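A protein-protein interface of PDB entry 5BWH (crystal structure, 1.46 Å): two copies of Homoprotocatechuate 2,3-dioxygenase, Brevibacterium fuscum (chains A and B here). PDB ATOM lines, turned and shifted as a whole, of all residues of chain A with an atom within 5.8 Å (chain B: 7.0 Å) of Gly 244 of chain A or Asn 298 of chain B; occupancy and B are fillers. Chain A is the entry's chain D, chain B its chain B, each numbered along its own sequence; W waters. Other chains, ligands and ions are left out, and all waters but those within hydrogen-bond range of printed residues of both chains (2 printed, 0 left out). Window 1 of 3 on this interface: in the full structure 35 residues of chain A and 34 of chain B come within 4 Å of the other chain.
Of the 19 printed residues of chain B, 3 touch a printed residue of chain A.
Printed residues of chain A that touch a printed residue of chain B: Cys 229, Ile 241, Glu 242, Gly 244 and Pro 245.
Hydrophobic or aromatic side chains of chain A within 4 Å of the printed part of chain B: Ile 241 and Pro 245.
Among the printed residues, no Asp or Glu carboxylate lies within 4 Å of a Lys or Arg side-chain nitrogen of the other chain.
The backbone carbonyl oxygen of Ile 241 of chain A lies within hydrogen-bond range of the side-chain amino group of Lys 357 of chain B, 2.9 Å away.
The side-chain amide nitrogen (ND2) of Asn 298 of chain B is in hydrogen-bond range of the backbone carbonyl oxygen (O) of Gly 244 of chain A.
Printed residues of chain B within 4 Å of Gly 244 of chain A: Asn 298.
Asn 298 of chain B touches just one residue of chain A: Gly 244 (3.1 Å).
Printed residues of chain B within 4 Å of Glu 242 of chain A: Lys 357.
Of the printed residues of chain B, Ile 241 of chain A touches Trp 296 (3.8 Å) and Lys 357 (2.9 Å).
Of the printed residues of chain A, Trp 296 of chain B touches Cys 229, Ile 241 and Pro 245.
Of the printed residues of chain A, Lys 357 of chain B touches Ile 241 (2.9 Å) and Glu 242 (3.9 Å).
Of the printed residues of chain B, Pro 245 of chain A touches Trp 296.
Water W2 bridges O of Pro 245 of chain B (2.8 Å) and O of Pro 245 of chain A (2.9 Å).
Water W1 lies within hydrogen-bond range of the side-chain amide oxygen of Asn 298 of chain B (2.9 Å) and the backbone NH of Gly 244 of chain A (2.9 Å).
Positions printed for both chains: 243, 244, 245, 246 and 255.
CB of Cys 229 of chain A touches NE1 of Trp 296 of chain B, at 3.3 Å.
Trp 296 of chain B touches Ile 241 of chain A.
Lys 357 of chain B touches Glu 242 of chain A (CD to O, 3.9 Å).
CZ3 of Trp 296 of chain B touches CD of Pro 245 of chain A (3.3 Å).
The side-chain amino group of Lys 357 of chain B lies within hydrogen-bond range of the backbone carbonyl oxygen of Trp 296 of chain B (3.0 Å).
N of Asn 298 of chain B sits at hydrogen-bond distance from OD1 of Asp 294 of chain B (3.0 Å).
OD1 of Asp 294 of chain B lies close to N of Trp 296 of chain B (3.2 Å).
N of Glu 242 of chain A lies within hydrogen-bond range of O of Tyr 257 of chain A (2.9 Å).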
ATOM      1  N   CYS A 229     -28.263  -1.840  20.755  1.00  0.00           N
ATOM      2  CA  CYS A 229     -28.480  -0.398  20.666  1.00  0.00           C
ATOM      3  C   CYS A 229     -28.537   0.091  19.224  1.00  0.00           C
ATOM      4  O   CYS A 229     -29.424   0.869  18.843  1.00  0.00           O
ATOM      5  CB  CYS A 229     -27.368   0.370  21.394  1.00  0.00           C
ATOM      6  SG  CYS A 229     -27.230   0.027  23.136  1.00  0.00           S
ATOM      7  N   ILE A 241     -34.615   2.533  24.481  1.00  0.00           N
ATOM      8  CA  ILE A 241     -33.372   2.348  25.228  1.00  0.00           C
ATOM      9  C   ILE A 241     -33.464   3.254  26.445  1.00  0.00           C
ATOM     10  O   ILE A 241     -33.488   4.476  26.319  1.00  0.00           O
ATOM     11  CB  ILE A 241     -32.141   2.734  24.398  1.00  0.00           C
ATOM     12  CG1 ILE A 241     -32.016   1.863  23.144  1.00  0.00           C
ATOM     13  CG2 ILE A 241     -30.882   2.660  25.248  1.00  0.00           C
ATOM     14  CD1 ILE A 241     -30.966   2.388  22.173  1.00  0.00           C
ATOM     15  N   GLU A 242     -33.566   2.655  27.622  1.00  0.00           N
ATOM     16  CA  GLU A 242     -33.777   3.442  28.840  1.00  0.00           C
ATOM     17  C   GLU A 242     -32.481   4.022  29.382  1.00  0.00           C
ATOM     18  O   GLU A 242     -32.417   5.189  29.759  1.00  0.00           O
ATOM     19  CB  GLU A 242     -34.434   2.622  29.941  1.00  0.00           C
ATOM     20  CG  GLU A 242     -34.864   3.484  31.126  1.00  0.00           C
ATOM     21  CD  GLU A 242     -35.225   2.657  32.350  1.00  0.00           C
ATOM     22  OE1 GLU A 242     -34.646   1.547  32.528  1.00  0.00           O
ATOM     23  OE2 GLU A 242     -36.070   3.141  33.147  1.00  0.00           O
ATOM     24  N   ARG A 243     -31.475   3.168  29.477  1.00  0.00           N
ATOM     25  CA  ARG A 243     -30.263   3.475  30.237  1.00  0.00           C
ATOM     26  C   ARG A 243     -29.105   2.647  29.703  1.00  0.00           C
ATOM     27  O   ARG A 243     -29.242   1.451  29.548  1.00  0.00           O
ATOM     28  CB  ARG A 243     -30.464   3.198  31.732  1.00  0.00           C
ATOM     29  CG  ARG A 243     -29.184   3.418  32.535  1.00  0.00           C
ATOM     30  CD  ARG A 243     -29.370   3.264  34.039  1.00  0.00           C
ATOM     31  NE  ARG A 243     -28.053   3.155  34.633  1.00  0.00           N
ATOM     32  CZ  ARG A 243     -27.699   2.346  35.618  1.00  0.00           C
ATOM     33  NH1 ARG A 243     -28.598   1.660  36.327  1.00  0.00           N
ATOM     34  NH2 ARG A 243     -26.419   2.257  35.913  1.00  0.00           N
ATOM     35  N   GLY A 244     -27.965   3.289  29.465  1.00  0.00           N
ATOM     36  CA  GLY A 244     -26.788   2.596  28.980  1.00  0.00           C
ATOM     37  C   GLY A 244     -26.521   2.856  27.518  1.00  0.00           C
ATOM     38  O   GLY A 244     -27.066   3.813  26.931  1.00  0.00           O
ATOM     39  N   PRO A 245     -25.640   2.054  26.912  1.00  0.00           N
ATOM     40  CA  PRO A 245     -24.855   1.001  27.538  1.00  0.00           C
ATOM     41  C   PRO A 245     -23.774   1.542  28.458  1.00  0.00           C
ATOM     42  O   PRO A 245     -23.383   2.713  28.376  1.00  0.00           O
ATOM     43  CB  PRO A 245     -24.249   0.281  26.347  1.00  0.00           C
ATOM     44  CG  PRO A 245     -24.070   1.357  25.320  1.00  0.00           C
ATOM     45  CD  PRO A 245     -25.211   2.306  25.527  1.00  0.00           C
ATOM     46  N   GLY A 246     -23.340   0.699  29.383  1.00  0.00           N
ATOM     47  CA  GLY A 246     -22.335   1.128  30.351  1.00  0.00           C
ATOM     48  C   GLY A 246     -21.560  -0.054  30.901  1.00  0.00           C
ATOM     49  O   GLY A 246     -21.800  -1.211  30.564  1.00  0.00           O
ATOM     50  N   TYR A 255     -23.444  -3.527  30.413  1.00  0.00           N
ATOM     51  CA  TYR A 255     -24.907  -3.567  30.560  1.00  0.00           C
ATOM     52  C   TYR A 255     -25.650  -2.612  29.654  1.00  0.00           C
ATOM     53  O   TYR A 255     -25.087  -1.643  29.132  1.00  0.00           O
ATOM     54  CB  TYR A 255     -25.304  -3.268  32.003  1.00  0.00           C
ATOM     55  CG  TYR A 255     -25.191  -1.816  32.378  1.00  0.00           C
ATOM     56  CD1 TYR A 255     -24.028  -1.302  32.930  1.00  0.00           C
ATOM     57  CD2 TYR A 255     -26.242  -0.930  32.135  1.00  0.00           C
ATOM     58  CE1 TYR A 255     -23.916   0.046  33.241  1.00  0.00           C
ATOM     59  CE2 TYR A 255     -26.137   0.433  32.416  1.00  0.00           C
ATOM     60  CZ  TYR A 255     -24.970   0.913  32.977  1.00  0.00           C
ATOM     61  OH  TYR A 255     -24.876   2.235  33.284  1.00  0.00           O
ATOM     62  N   LEU A 256     -26.952  -2.896  29.546  1.00  0.00           N
ATOM     63  CA  LEU A 256     -27.909  -2.064  28.844  1.00  0.00           C
ATOM     64  C   LEU A 256     -29.294  -2.344  29.439  1.00  0.00           C
ATOM     65  O   LEU A 256     -29.595  -3.510  29.715  1.00  0.00           O
ATOM     66  CB  LEU A 256     -27.925  -2.461  27.380  1.00  0.00           C
ATOM     67  CG  LEU A 256     -28.952  -1.778  26.477  1.00  0.00           C
ATOM     68  CD1 LEU A 256     -28.615  -0.317  26.324  1.00  0.00           C
ATOM     69  CD2 LEU A 256     -28.988  -2.437  25.118  1.00  0.00           C
ATOM     70  N   TYR A 257     -30.131  -1.310  29.565  1.00  0.00           N
ATOM     71  CA  TYR A 257     -31.540  -1.499  29.932  1.00  0.00           C
ATOM     72  C   TYR A 257     -32.457  -0.965  28.854  1.00  0.00           C
ATOM     73  O   TYR A 257     -32.324   0.175  28.403  1.00  0.00           O
ATOM     74  CB  TYR A 257     -31.867  -0.783  31.231  1.00  0.00           C
ATOM     75  CG  TYR A 257     -31.062  -1.261  32.405  1.00  0.00           C
ATOM     76  CD1 TYR A 257     -31.473  -2.382  33.174  1.00  0.00           C
ATOM     77  CD2 TYR A 257     -29.890  -0.602  32.775  1.00  0.00           C
ATOM     78  CE1 TYR A 257     -30.730  -2.823  34.270  1.00  0.00           C
ATOM     79  CE2 TYR A 257     -29.150  -1.052  33.856  1.00  0.00           C
ATOM     80  CZ  TYR A 257     -29.556  -2.144  34.594  1.00  0.00           C
ATOM     81  OH  TYR A 257     -28.802  -2.531  35.668  1.00  0.00           O
ATOM     82  N   ARG B 243     -18.569  12.881  27.560  1.00  0.00           N
ATOM     83  CA  ARG B 243     -19.728  12.416  26.808  1.00  0.00           C
ATOM     84  C   ARG B 243     -19.401  11.095  26.125  1.00  0.00           C
ATOM     85  O   ARG B 243     -18.334  10.922  25.540  1.00  0.00           O
ATOM     86  CB  ARG B 243     -20.118  13.490  25.771  1.00  0.00           C
ATOM     87  CG  ARG B 243     -21.227  13.080  24.827  1.00  0.00           C
ATOM     88  CD  ARG B 243     -21.552  14.151  23.800  1.00  0.00           C
ATOM     89  NE  ARG B 243     -22.321  13.465  22.770  1.00  0.00           N
ATOM     90  CZ  ARG B 243     -22.265  13.697  21.468  1.00  0.00           C
ATOM     91  NH1 ARG B 243     -21.601  14.746  20.986  1.00  0.00           N
ATOM     92  NH2 ARG B 243     -22.916  12.877  20.643  1.00  0.00           N
ATOM     93  N   GLY B 244     -20.331  10.157  26.219  1.00  0.00           N
ATOM     94  CA  GLY B 244     -20.180   8.869  25.587  1.00  0.00           C
ATOM     95  C   GLY B 244     -19.929   7.778  26.613  1.00  0.00           C
ATOM     96  O   GLY B 244     -20.081   7.992  27.819  1.00  0.00           O
ATOM     97  N   PRO B 245     -19.523   6.587  26.144  1.00  0.00           N
ATOM     98  CA  PRO B 245     -19.355   6.252  24.757  1.00  0.00           C
ATOM     99  C   PRO B 245     -20.696   6.093  24.046  1.00  0.00           C
ATOM    100  O   PRO B 245     -21.738   5.895  24.689  1.00  0.00           O
ATOM    101  CB  PRO B 245     -18.587   4.920  24.809  1.00  0.00           C
ATOM    102  CG  PRO B 245     -19.122   4.285  26.046  1.00  0.00           C
ATOM    103  CD  PRO B 245     -19.303   5.419  27.013  1.00  0.00           C
ATOM    104  N   GLY B 246     -20.658   6.208  22.723  1.00  0.00           N
ATOM    105  CA  GLY B 246     -21.869   6.114  21.927  1.00  0.00           C
ATOM    106  C   GLY B 246     -21.608   5.710  20.500  1.00  0.00           C
ATOM    107  O   GLY B 246     -20.465   5.487  20.092  1.00  0.00           O
ATOM    108  N   TYR B 255     -17.770   6.265  19.444  1.00  0.00           N
ATOM    109  CA  TYR B 255     -17.077   7.459  19.909  1.00  0.00           C
ATOM    110  C   TYR B 255     -17.051   7.602  21.421  1.00  0.00           C
ATOM    111  O   TYR B 255     -17.849   6.983  22.144  1.00  0.00           O
ATOM    112  CB  TYR B 255     -17.724   8.715  19.306  1.00  0.00           C
ATOM    113  CG  TYR B 255     -19.059   9.066  19.937  1.00  0.00           C
ATOM    114  CD1 TYR B 255     -20.260   8.621  19.370  1.00  0.00           C
ATOM    115  CD2 TYR B 255     -19.132   9.845  21.097  1.00  0.00           C
ATOM    116  CE1 TYR B 255     -21.483   8.947  19.962  1.00  0.00           C
ATOM    117  CE2 TYR B 255     -20.345  10.177  21.682  1.00  0.00           C
ATOM    118  CZ  TYR B 255     -21.528   9.749  21.099  1.00  0.00           C
ATOM    119  OH  TYR B 255     -22.733  10.081  21.702  1.00  0.00           O
ATOM    120  N   ASN B 290     -33.223  13.359  17.181  1.00  0.00           N
ATOM    121  CA  ASN B 290     -32.514  12.945  18.373  1.00  0.00           C
ATOM    122  C   ASN B 290     -31.559  11.752  18.198  1.00  0.00           C
ATOM    123  O   ASN B 290     -30.896  11.378  19.160  1.00  0.00           O
ATOM    124  CB  ASN B 290     -33.495  12.597  19.510  1.00  0.00           C
ATOM    125  CG  ASN B 290     -32.808  12.488  20.844  1.00  0.00           C
ATOM    126  OD1 ASN B 290     -32.092  13.408  21.270  1.00  0.00           O
ATOM    127  ND2 ASN B 290     -33.026  11.373  21.521  1.00  0.00           N
ATOM    128  N   GLN B 291     -31.485  11.193  16.992  1.00  0.00           N
ATOM    129  CA  GLN B 291     -30.480  10.185  16.659  1.00  0.00           C
ATOM    130  C   GLN B 291     -29.305  10.700  15.837  1.00  0.00           C
ATOM    131  O   GLN B 291     -28.457   9.907  15.438  1.00  0.00           O
ATOM    132  CB  GLN B 291     -31.129   8.952  15.989  1.00  0.00           C
ATOM    133  CG  GLN B 291     -32.175   8.252  16.861  1.00  0.00           C
ATOM    134  CD  GLN B 291     -32.744   6.945  16.300  1.00  0.00           C
ATOM    135  OE1 GLN B 291     -33.651   6.353  16.899  1.00  0.00           O
ATOM    136  NE2 GLN B 291     -32.216   6.470  15.171  1.00  0.00           N
ATOM    137  N   ARG B 293     -26.727  12.829  16.609  1.00  0.00           N
ATOM    138  CA  ARG B 293     -25.418  12.980  17.270  1.00  0.00           C
ATOM    139  C   ARG B 293     -25.060  11.713  18.028  1.00  0.00           C
ATOM    140  O   ARG B 293     -23.991  11.140  17.839  1.00  0.00           O
ATOM    141  CB  ARG B 293     -25.374  14.217  18.166  1.00  0.00           C
ATOM    142  CG  ARG B 293     -25.178  15.491  17.337  1.00  0.00           C
ATOM    143  CD  ARG B 293     -24.655  16.659  18.151  1.00  0.00           C
ATOM    144  NE  ARG B 293     -24.457  17.867  17.337  1.00  0.00           N
ATOM    145  CZ  ARG B 293     -23.360  18.138  16.621  1.00  0.00           C
ATOM    146  NH1 ARG B 293     -22.345  17.284  16.537  1.00  0.00           N
ATOM    147  NH2 ARG B 293     -23.283  19.269  15.946  1.00  0.00           N
ATOM    148  N   ASP B 294     -25.989  11.272  18.858  1.00  0.00           N
ATOM    149  CA  ASP B 294     -25.974   9.926  19.428  1.00  0.00           C
ATOM    150  C   ASP B 294     -27.147   9.127  18.851  1.00  0.00           C
ATOM    151  O   ASP B 294     -28.320   9.442  19.094  1.00  0.00           O
ATOM    152  CB  ASP B 294     -26.062   9.965  20.943  1.00  0.00           C
ATOM    153  CG  ASP B 294     -25.793   8.612  21.548  1.00  0.00           C
ATOM    154  OD1 ASP B 294     -26.768   7.891  21.854  1.00  0.00           O
ATOM    155  OD2 ASP B 294     -24.595   8.261  21.663  1.00  0.00           O
ATOM    156  N   TRP B 295     -26.807   8.095  18.099  1.00  0.00           N
ATOM    157  CA  TRP B 295     -27.761   7.245  17.373  1.00  0.00           C
ATOM    158  C   TRP B 295     -28.724   6.534  18.313  1.00  0.00           C
ATOM    159  O   TRP B 295     -29.838   6.190  17.926  1.00  0.00           O
ATOM    160  CB  TRP B 295     -26.963   6.216  16.597  1.00  0.00           C
ATOM    161  CG  TRP B 295     -27.663   5.222  15.753  1.00  0.00           C
ATOM    162  CD1 TRP B 295     -27.597   3.867  15.877  1.00  0.00           C
ATOM    163  CD2 TRP B 295     -28.476   5.477  14.583  1.00  0.00           C
ATOM    164  NE1 TRP B 295     -28.308   3.252  14.862  1.00  0.00           N
ATOM    165  CE2 TRP B 295     -28.867   4.221  14.071  1.00  0.00           C
ATOM    166  CE3 TRP B 295     -28.904   6.645  13.924  1.00  0.00           C
ATOM    167  CZ2 TRP B 295     -29.636   4.099  12.906  1.00  0.00           C
ATOM    168  CZ3 TRP B 295     -29.674   6.508  12.780  1.00  0.00           C
ATOM    169  CH2 TRP B 295     -30.036   5.244  12.296  1.00  0.00           C
ATOM    170  N   TRP B 296     -28.289   6.312  19.549  1.00  0.00           N
ATOM    171  CA  TRP B 296     -29.097   5.630  20.551  1.00  0.00           C
ATOM    172  C   TRP B 296     -30.004   6.613  21.313  1.00  0.00           C
ATOM    173  O   TRP B 296     -30.725   6.219  22.251  1.00  0.00           O
ATOM    174  CB  TRP B 296     -28.169   4.928  21.533  1.00  0.00           C
ATOM    175  CG  TRP B 296     -27.190   4.021  20.876  1.00  0.00           C
ATOM    176  CD1 TRP B 296     -27.313   3.398  19.655  1.00  0.00           C
ATOM    177  CD2 TRP B 296     -25.897   3.653  21.383  1.00  0.00           C
ATOM    178  NE1 TRP B 296     -26.188   2.654  19.390  1.00  0.00           N
ATOM    179  CE2 TRP B 296     -25.308   2.790  20.436  1.00  0.00           C
ATOM    180  CE3 TRP B 296     -25.181   3.976  22.547  1.00  0.00           C
ATOM    181  CZ2 TRP B 296     -24.033   2.252  20.615  1.00  0.00           C
ATOM    182  CZ3 TRP B 296     -23.929   3.438  22.722  1.00  0.00           C
ATOM    183  CH2 TRP B 296     -23.374   2.582  21.780  1.00  0.00           C
ATOM    184  N   GLY B 297     -29.922   7.896  20.948  1.00  0.00           N
ATOM    185  CA  GLY B 297     -30.737   8.917  21.549  1.00  0.00           C
ATOM    186  C   GLY B 297     -30.290   9.446  22.885  1.00  0.00           C
ATOM    187  O   GLY B 297     -31.013  10.224  23.505  1.00  0.00           O
ATOM    188  N   ASN B 298     -29.102   9.057  23.334  1.00  0.00           N
ATOM    189  CA  ASN B 298     -28.591   9.621  24.566  1.00  0.00           C
ATOM    190  C   ASN B 298     -28.399  11.137  24.439  1.00  0.00           C
ATOM    191  O   ASN B 298     -28.056  11.639  23.360  1.00  0.00           O
ATOM    192  CB  ASN B 298     -27.311   8.901  25.013  1.00  0.00           C
ATOM    193  CG  ASN B 298     -27.613   7.555  25.664  1.00  0.00           C
ATOM    194  OD1 ASN B 298     -28.615   7.415  26.360  1.00  0.00           O
ATOM    195  ND2 ASN B 298     -26.744   6.568  25.458  1.00  0.00           N
ATOM    196  N   PRO B 299     -28.645  11.874  25.542  1.00  0.00           N
ATOM    197  CA  PRO B 299     -28.621  13.319  25.449  1.00  0.00           C
ATOM    198  C   PRO B 299     -27.199  13.859  25.309  1.00  0.00           C
ATOM    199  O   PRO B 299     -26.242  13.268  25.806  1.00  0.00           O
ATOM    200  CB  PRO B 299     -29.288  13.760  26.759  1.00  0.00           C
ATOM    201  CG  PRO B 299     -28.978  12.664  27.704  1.00  0.00           C
ATOM    202  CD  PRO B 299     -29.058  11.424  26.885  1.00  0.00           C
ATOM    203  N   VAL B 300     -27.071  14.959  24.583  1.00  0.00           N
ATOM    204  CA  VAL B 300     -25.777  15.619  24.397  1.00  0.00           C
ATOM    205  C   VAL B 300     -25.576  16.591  25.549  1.00  0.00           C
ATOM    206  O   VAL B 300     -26.366  17.511  25.739  1.00  0.00           O
ATOM    207  CB  VAL B 300     -25.689  16.353  23.044  1.00  0.00           C
ATOM    208  CG1 VAL B 300     -24.366  17.089  22.894  1.00  0.00           C
ATOM    209  CG2 VAL B 300     -25.895  15.365  21.916  1.00  0.00           C
ATOM    210  N   VAL B 301     -24.504  16.372  26.315  1.00  0.00           N
ATOM    211  CA  VAL B 301     -24.219  17.166  27.489  1.00  0.00           C
ATOM    212  C   VAL B 301     -23.987  18.632  27.082  1.00  0.00           C
ATOM    213  O   VAL B 301     -23.348  18.906  26.057  1.00  0.00           O
ATOM    214  CB  VAL B 301     -23.020  16.575  28.286  1.00  0.00           C
ATOM    215  CG1 VAL B 301     -23.200  15.069  28.517  1.00  0.00           C
ATOM    216  CG2 VAL B 301     -21.728  16.792  27.561  1.00  0.00           C
ATOM    217  N   SER B 356     -33.367  14.305  26.113  1.00  0.00           N
ATOM    218  CA  SER B 356     -33.849  12.929  26.118  1.00  0.00           C
ATOM    219  C   SER B 356     -33.539  12.219  27.435  1.00  0.00           C
ATOM    220  O   SER B 356     -32.733  12.712  28.256  1.00  0.00           O
ATOM    221  CB  SER B 356     -33.227  12.154  24.967  1.00  0.00           C
ATOM    222  OG  SER B 356     -31.814  12.198  25.075  1.00  0.00           O
ATOM    223  N   LYS B 357     -34.182  11.069  27.616  1.00  0.00           N
ATOM    224  CA  LYS B 357     -33.860  10.107  28.682  1.00  0.00           C
ATOM    225  C   LYS B 357     -34.102  10.650  30.093  1.00  0.00           C
ATOM    226  O   LYS B 357     -33.582  10.112  31.063  1.00  0.00           O
ATOM    227  CB  LYS B 357     -32.419   9.539  28.561  1.00  0.00           C
ATOM    228  CG  LYS B 357     -32.007   9.121  27.165  1.00  0.00           C
ATOM    229  CD  LYS B 357     -32.376   7.708  26.778  1.00  0.00           C
ATOM    230  CE  LYS B 357     -31.750   7.359  25.427  1.00  0.00           C
ATOM    231  NZ  LYS B 357     -32.689   6.620  24.545  1.00  0.00           N
ATOM    232  N   PHE B 359     -33.776  13.872  31.414  1.00  0.00           N
ATOM    233  CA  PHE B 359     -32.900  14.917  31.908  1.00  0.00           C
ATOM    234  C   PHE B 359     -33.271  16.307  31.385  1.00  0.00           C
ATOM    235  O   PHE B 359     -33.875  16.446  30.311  1.00  0.00           O
ATOM    236  CB  PHE B 359     -31.468  14.595  31.548  1.00  0.00           C
ATOM    237  CG  PHE B 359     -30.941  13.366  32.225  1.00  0.00           C
ATOM    238  CD1 PHE B 359     -30.818  13.307  33.601  1.00  0.00           C
ATOM    239  CD2 PHE B 359     -30.564  12.256  31.468  1.00  0.00           C
ATOM    240  CE1 PHE B 359     -30.299  12.160  34.222  1.00  0.00           C
ATOM    241  CE2 PHE B 359     -30.051  11.133  32.075  1.00  0.00           C
ATOM    242  CZ  PHE B 359     -29.941  11.078  33.453  1.00  0.00           C
HETATM  243  O   HOH W   1     -28.276   6.129  28.932  1.00  0.00           O
HETATM  244  O   HOH W   2     -23.038   5.242  27.053  1.00  0.00           O
